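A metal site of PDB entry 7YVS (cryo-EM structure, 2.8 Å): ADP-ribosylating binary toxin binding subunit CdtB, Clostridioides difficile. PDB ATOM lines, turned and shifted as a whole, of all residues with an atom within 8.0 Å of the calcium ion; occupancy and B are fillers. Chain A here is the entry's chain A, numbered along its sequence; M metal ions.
N of Ser 445 is in hydrogen-bond range of O of Asp 440 (2.4 Å). N of Leu 442 sits close to OD2 of Asp 533. The side-chain amide nitrogen (ND2) of Asn 420 is in hydrogen-bond range of the side-chain carboxylate (OD1) of Asp 423, at 3.1 Å.
The side-chain hydroxyl (OG) of Ser 445 is bound to the calcium ion (2.4 Å). The calcium ion is bound by OD2 of Asp 533, at 2.5 Å. The calcium ion is bound by OD1 of Asp 533 (2.6 Å). The calcium ion is bound by O of Asn 420. OD2 of Asp 422 binds the calcium ion, 2.8 Å away. The calcium ion has five donor atoms within binding distance.
Merely in contact with the calcium ion: Gln 443.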
ATOM      1  N   PHE A 418     -11.720   5.712  13.300  1.00  0.00           N
ATOM      2  CA  PHE A 418     -10.796   5.880  12.185  1.00  0.00           C
ATOM      3  C   PHE A 418     -11.329   5.128  10.972  1.00  0.00           C
ATOM      4  O   PHE A 418     -12.013   4.118  11.112  1.00  0.00           O
ATOM      5  CB  PHE A 418      -9.394   5.383  12.566  1.00  0.00           C
ATOM      6  CG  PHE A 418      -8.446   5.275  11.406  1.00  0.00           C
ATOM      7  CD1 PHE A 418      -7.791   6.386  10.923  1.00  0.00           C
ATOM      8  CD2 PHE A 418      -8.208   4.053  10.803  1.00  0.00           C
ATOM      9  CE1 PHE A 418      -6.929   6.296   9.859  1.00  0.00           C
ATOM     10  CE2 PHE A 418      -7.334   3.952   9.742  1.00  0.00           C
ATOM     11  CZ  PHE A 418      -6.694   5.074   9.270  1.00  0.00           C
ATOM     12  N   THR A 419     -11.002   5.641   9.797  1.00  0.00           N
ATOM     13  CA  THR A 419     -11.376   4.995   8.542  1.00  0.00           C
ATOM     14  C   THR A 419     -10.393   5.380   7.452  1.00  0.00           C
ATOM     15  O   THR A 419      -9.932   6.523   7.383  1.00  0.00           O
ATOM     16  CB  THR A 419     -12.810   5.346   8.129  1.00  0.00           C
ATOM     17  OG1 THR A 419     -13.125   4.692   6.898  1.00  0.00           O
ATOM     18  CG2 THR A 419     -12.964   6.860   7.968  1.00  0.00           C
ATOM     19  N   ASN A 420     -10.065   4.409   6.605  1.00  0.00           N
ATOM     20  CA  ASN A 420      -9.203   4.621   5.449  1.00  0.00           C
ATOM     21  C   ASN A 420      -9.944   4.442   4.129  1.00  0.00           C
ATOM     22  O   ASN A 420      -9.325   4.519   3.068  1.00  0.00           O
ATOM     23  CB  ASN A 420      -8.010   3.658   5.495  1.00  0.00           C
ATOM     24  CG  ASN A 420      -8.430   2.220   5.728  1.00  0.00           C
ATOM     25  OD1 ASN A 420      -9.616   1.914   5.784  1.00  0.00           O
ATOM     26  ND2 ASN A 420      -7.454   1.339   5.864  1.00  0.00           N
ATOM     27  N   PHE A 421     -11.251   4.194   4.188  1.00  0.00           N
ATOM     28  CA  PHE A 421     -12.138   4.009   3.041  1.00  0.00           C
ATOM     29  C   PHE A 421     -11.744   2.814   2.182  1.00  0.00           C
ATOM     30  O   PHE A 421     -12.234   2.696   1.048  1.00  0.00           O
ATOM     31  CB  PHE A 421     -12.216   5.270   2.175  1.00  0.00           C
ATOM     32  CG  PHE A 421     -12.209   6.545   2.953  1.00  0.00           C
ATOM     33  CD1 PHE A 421     -13.090   6.739   4.001  1.00  0.00           C
ATOM     34  CD2 PHE A 421     -11.321   7.561   2.626  1.00  0.00           C
ATOM     35  CE1 PHE A 421     -13.076   7.923   4.720  1.00  0.00           C
ATOM     36  CE2 PHE A 421     -11.317   8.742   3.343  1.00  0.00           C
ATOM     37  CZ  PHE A 421     -12.185   8.926   4.393  1.00  0.00           C
ATOM     38  N   ASP A 422     -10.893   1.924   2.673  1.00  0.00           N
ATOM     39  CA  ASP A 422     -10.468   0.747   1.912  1.00  0.00           C
ATOM     40  C   ASP A 422     -10.966  -0.544   2.545  1.00  0.00           C
ATOM     41  O   ASP A 422     -11.687  -1.313   1.905  1.00  0.00           O
ATOM     42  CB  ASP A 422      -8.946   0.723   1.773  1.00  0.00           C
ATOM     43  CG  ASP A 422      -8.422   1.826   0.877  1.00  0.00           C
ATOM     44  OD1 ASP A 422      -8.897   1.909  -0.283  1.00  0.00           O
ATOM     45  OD2 ASP A 422      -7.556   2.602   1.314  1.00  0.00           O
ATOM     46  N   ASP A 423     -10.578  -0.827   3.793  1.00  0.00           N
ATOM     47  CA  ASP A 423     -11.058  -2.006   4.494  1.00  0.00           C
ATOM     48  C   ASP A 423     -11.409  -1.764   5.949  1.00  0.00           C
ATOM     49  O   ASP A 423     -12.078  -2.628   6.536  1.00  0.00           O
ATOM     50  CB  ASP A 423     -10.031  -3.136   4.403  1.00  0.00           C
ATOM     51  CG  ASP A 423      -8.653  -2.709   4.862  1.00  0.00           C
ATOM     52  OD1 ASP A 423      -8.434  -1.482   5.038  1.00  0.00           O
ATOM     53  OD2 ASP A 423      -7.780  -3.589   5.058  1.00  0.00           O
ATOM     54  N   THR A 436     -15.582   6.033  -2.834  1.00  0.00           N
ATOM     55  CA  THR A 436     -14.286   5.311  -2.749  1.00  0.00           C
ATOM     56  C   THR A 436     -14.202   4.292  -3.888  1.00  0.00           C
ATOM     57  O   THR A 436     -14.567   3.117  -3.686  1.00  0.00           O
ATOM     58  CB  THR A 436     -14.036   4.733  -1.342  1.00  0.00           C
ATOM     59  OG1 THR A 436     -12.927   3.842  -1.429  1.00  0.00           O
ATOM     60  CG2 THR A 436     -15.229   4.011  -0.758  1.00  0.00           C
ATOM     61  N   ASN A 438     -11.651   5.252  -6.523  1.00  0.00           N
ATOM     62  CA  ASN A 438     -10.423   5.644  -7.185  1.00  0.00           C
ATOM     63  C   ASN A 438      -9.205   5.082  -6.455  1.00  0.00           C
ATOM     64  O   ASN A 438      -9.299   4.563  -5.342  1.00  0.00           O
ATOM     65  CB  ASN A 438     -10.332   7.170  -7.277  1.00  0.00           C
ATOM     66  CG  ASN A 438     -10.547   7.859  -5.944  1.00  0.00           C
ATOM     67  OD1 ASN A 438     -10.784   7.199  -4.922  1.00  0.00           O
ATOM     68  ND2 ASN A 438     -10.471   9.181  -5.937  1.00  0.00           N
ATOM     69  N   GLN A 439      -8.047   5.200  -7.099  1.00  0.00           N
ATOM     70  CA  GLN A 439      -6.799   4.718  -6.536  1.00  0.00           C
ATOM     71  C   GLN A 439      -5.933   5.839  -5.974  1.00  0.00           C
ATOM     72  O   GLN A 439      -4.727   5.676  -5.839  1.00  0.00           O
ATOM     73  CB  GLN A 439      -6.002   3.935  -7.596  1.00  0.00           C
ATOM     74  CG  GLN A 439      -6.688   2.648  -8.024  1.00  0.00           C
ATOM     75  CD  GLN A 439      -6.917   1.694  -6.869  1.00  0.00           C
ATOM     76  OE1 GLN A 439      -8.050   1.494  -6.426  1.00  0.00           O
ATOM     77  NE2 GLN A 439      -5.833   1.115  -6.362  1.00  0.00           N
ATOM     78  N   ASP A 440      -6.539   6.982  -5.657  1.00  0.00           N
ATOM     79  CA  ASP A 440      -5.822   8.063  -4.992  1.00  0.00           C
ATOM     80  C   ASP A 440      -5.837   7.853  -3.486  1.00  0.00           C
ATOM     81  O   ASP A 440      -6.478   6.940  -2.955  1.00  0.00           O
ATOM     82  CB  ASP A 440      -6.430   9.408  -5.361  1.00  0.00           C
ATOM     83  CG  ASP A 440      -6.272   9.738  -6.830  1.00  0.00           C
ATOM     84  OD1 ASP A 440      -5.177   9.487  -7.369  1.00  0.00           O
ATOM     85  OD2 ASP A 440      -7.238  10.247  -7.430  1.00  0.00           O
ATOM     86  N   GLY A 441      -5.130   8.726  -2.772  1.00  0.00           N
ATOM     87  CA  GLY A 441      -5.014   8.631  -1.329  1.00  0.00           C
ATOM     88  C   GLY A 441      -3.750   7.910  -0.920  1.00  0.00           C
ATOM     89  O   GLY A 441      -2.942   7.455  -1.735  1.00  0.00           O
ATOM     90  N   LEU A 442      -3.585   7.803   0.403  1.00  0.00           N
ATOM     91  CA  LEU A 442      -2.397   7.154   0.939  1.00  0.00           C
ATOM     92  C   LEU A 442      -2.376   5.671   0.624  1.00  0.00           C
ATOM     93  O   LEU A 442      -1.305   5.086   0.464  1.00  0.00           O
ATOM     94  CB  LEU A 442      -2.310   7.369   2.452  1.00  0.00           C
ATOM     95  CG  LEU A 442      -1.692   8.664   2.994  1.00  0.00           C
ATOM     96  CD1 LEU A 442      -0.227   8.783   2.575  1.00  0.00           C
ATOM     97  CD2 LEU A 442      -2.474   9.903   2.574  1.00  0.00           C
ATOM     98  N   GLN A 443      -3.549   5.031   0.538  1.00  0.00           N
ATOM     99  CA  GLN A 443      -3.597   3.595   0.276  1.00  0.00           C
ATOM    100  C   GLN A 443      -4.701   3.197  -0.695  1.00  0.00           C
ATOM    101  O   GLN A 443      -5.161   2.049  -0.663  1.00  0.00           O
ATOM    102  CB  GLN A 443      -3.756   2.826   1.587  1.00  0.00           C
ATOM    103  CG  GLN A 443      -2.471   2.700   2.396  1.00  0.00           C
ATOM    104  CD  GLN A 443      -2.291   3.848   3.371  1.00  0.00           C
ATOM    105  OE1 GLN A 443      -3.241   4.519   3.743  1.00  0.00           O
ATOM    106  NE2 GLN A 443      -1.044   4.070   3.787  1.00  0.00           N
ATOM    107  N   GLY A 444      -5.161   4.109  -1.548  1.00  0.00           N
ATOM    108  CA  GLY A 444      -6.105   3.761  -2.595  1.00  0.00           C
ATOM    109  C   GLY A 444      -7.550   4.156  -2.358  1.00  0.00           C
ATOM    110  O   GLY A 444      -8.442   3.416  -2.769  1.00  0.00           O
ATOM    111  N   SER A 445      -7.801   5.301  -1.723  1.00  0.00           N
ATOM    112  CA  SER A 445      -9.170   5.767  -1.509  1.00  0.00           C
ATOM    113  C   SER A 445      -9.132   7.241  -1.172  1.00  0.00           C
ATOM    114  O   SER A 445      -8.267   7.684  -0.402  1.00  0.00           O
ATOM    115  CB  SER A 445      -9.843   4.975  -0.392  1.00  0.00           C
ATOM    116  OG  SER A 445      -9.152   5.117   0.836  1.00  0.00           O
ATOM    117  N   ALA A 446     -10.048   7.994  -1.733  1.00  0.00           N
ATOM    118  CA  ALA A 446     -10.068   9.437  -1.496  1.00  0.00           C
ATOM    119  C   ALA A 446     -11.450   9.975  -1.153  1.00  0.00           C
ATOM    120  O   ALA A 446     -11.547  11.056  -0.556  1.00  0.00           O
ATOM    121  CB  ALA A 446      -9.511  10.168  -2.717  1.00  0.00           C
ATOM    122  N   ASN A 447     -12.513   9.295  -1.575  1.00  0.00           N
ATOM    123  CA  ASN A 447     -13.926   9.597  -1.339  1.00  0.00           C
ATOM    124  C   ASN A 447     -14.246  11.090  -1.282  1.00  0.00           C
ATOM    125  O   ASN A 447     -14.925  11.558  -0.372  1.00  0.00           O
ATOM    126  CB  ASN A 447     -14.459   8.871  -0.096  1.00  0.00           C
ATOM    127  CG  ASN A 447     -13.973   9.454   1.227  1.00  0.00           C
ATOM    128  OD1 ASN A 447     -13.124  10.336   1.280  1.00  0.00           O
ATOM    129  ND2 ASN A 447     -14.556   8.962   2.312  1.00  0.00           N
ATOM    130  N   TYR A 503       0.505  15.062   0.467  1.00  0.00           N
ATOM    131  CA  TYR A 503      -0.477  14.788   1.503  1.00  0.00           C
ATOM    132  C   TYR A 503       0.053  15.294   2.844  1.00  0.00           C
ATOM    133  O   TYR A 503       1.171  14.946   3.237  1.00  0.00           O
ATOM    134  CB  TYR A 503      -0.786  13.297   1.584  1.00  0.00           C
ATOM    135  CG  TYR A 503      -2.022  12.880   0.818  1.00  0.00           C
ATOM    136  CD1 TYR A 503      -3.285  13.254   1.250  1.00  0.00           C
ATOM    137  CD2 TYR A 503      -1.928  12.104  -0.329  1.00  0.00           C
ATOM    138  CE1 TYR A 503      -4.417  12.881   0.570  1.00  0.00           C
ATOM    139  CE2 TYR A 503      -3.063  11.717  -1.027  1.00  0.00           C
ATOM    140  CZ  TYR A 503      -4.304  12.110  -0.572  1.00  0.00           C
ATOM    141  OH  TYR A 503      -5.437  11.737  -1.253  1.00  0.00           O
ATOM    142  N   LEU A 532      -9.248  13.471   0.249  1.00  0.00           N
ATOM    143  CA  LEU A 532      -9.161  13.246   1.678  1.00  0.00           C
ATOM    144  C   LEU A 532      -8.899  11.770   1.946  1.00  0.00           C
ATOM    145  O   LEU A 532      -9.274  10.909   1.148  1.00  0.00           O
ATOM    146  CB  LEU A 532     -10.440  13.685   2.399  1.00  0.00           C
ATOM    147  CG  LEU A 532     -10.660  15.184   2.543  1.00  0.00           C
ATOM    148  CD1 LEU A 532     -11.954  15.472   3.289  1.00  0.00           C
ATOM    149  CD2 LEU A 532      -9.472  15.831   3.254  1.00  0.00           C
ATOM    150  N   ASP A 533      -8.249  11.483   3.073  1.00  0.00           N
ATOM    151  CA  ASP A 533      -7.934  10.117   3.441  1.00  0.00           C
ATOM    152  C   ASP A 533      -7.589  10.047   4.920  1.00  0.00           C
ATOM    153  O   ASP A 533      -7.128  11.040   5.506  1.00  0.00           O
ATOM    154  CB  ASP A 533      -6.782   9.550   2.597  1.00  0.00           C
ATOM    155  CG  ASP A 533      -6.939   8.074   2.301  1.00  0.00           C
ATOM    156  OD1 ASP A 533      -7.924   7.466   2.778  1.00  0.00           O
ATOM    157  OD2 ASP A 533      -6.083   7.518   1.584  1.00  0.00           O
ATOM    158  N   ASN A 534      -7.812   8.870   5.508  1.00  0.00           N
ATOM    159  CA  ASN A 534      -7.409   8.557   6.874  1.00  0.00           C
ATOM    160  C   ASN A 534      -7.918   9.601   7.878  1.00  0.00           C
ATOM    161  O   ASN A 534      -7.152  10.309   8.524  1.00  0.00           O
ATOM    162  CB  ASN A 534      -5.885   8.407   6.972  1.00  0.00           C
ATOM    163  CG  ASN A 534      -5.356   7.274   6.112  1.00  0.00           C
ATOM    164  OD1 ASN A 534      -6.035   6.279   5.901  1.00  0.00           O
ATOM    165  ND2 ASN A 534      -4.135   7.431   5.622  1.00  0.00           N
ATOM    166  N   LEU A 535      -9.240   9.675   7.989  1.00  0.00           N
ATOM    167  CA  LEU A 535      -9.867  10.576   8.960  1.00  0.00           C
ATOM    168  C   LEU A 535      -9.993   9.858  10.301  1.00  0.00           C
ATOM    169  O   LEU A 535     -10.502   8.741  10.367  1.00  0.00           O
ATOM    170  CB  LEU A 535     -11.225  11.037   8.461  1.00  0.00           C
ATOM    171  CG  LEU A 535     -11.241  12.181   7.444  1.00  0.00           C
ATOM    172  CD1 LEU A 535     -10.771  11.731   6.073  1.00  0.00           C
ATOM    173  CD2 LEU A 535     -12.628  12.793   7.351  1.00  0.00           C
HETATM  174 CA    CA M   1      -6.956   5.245   1.907  1.00  0.00          CA
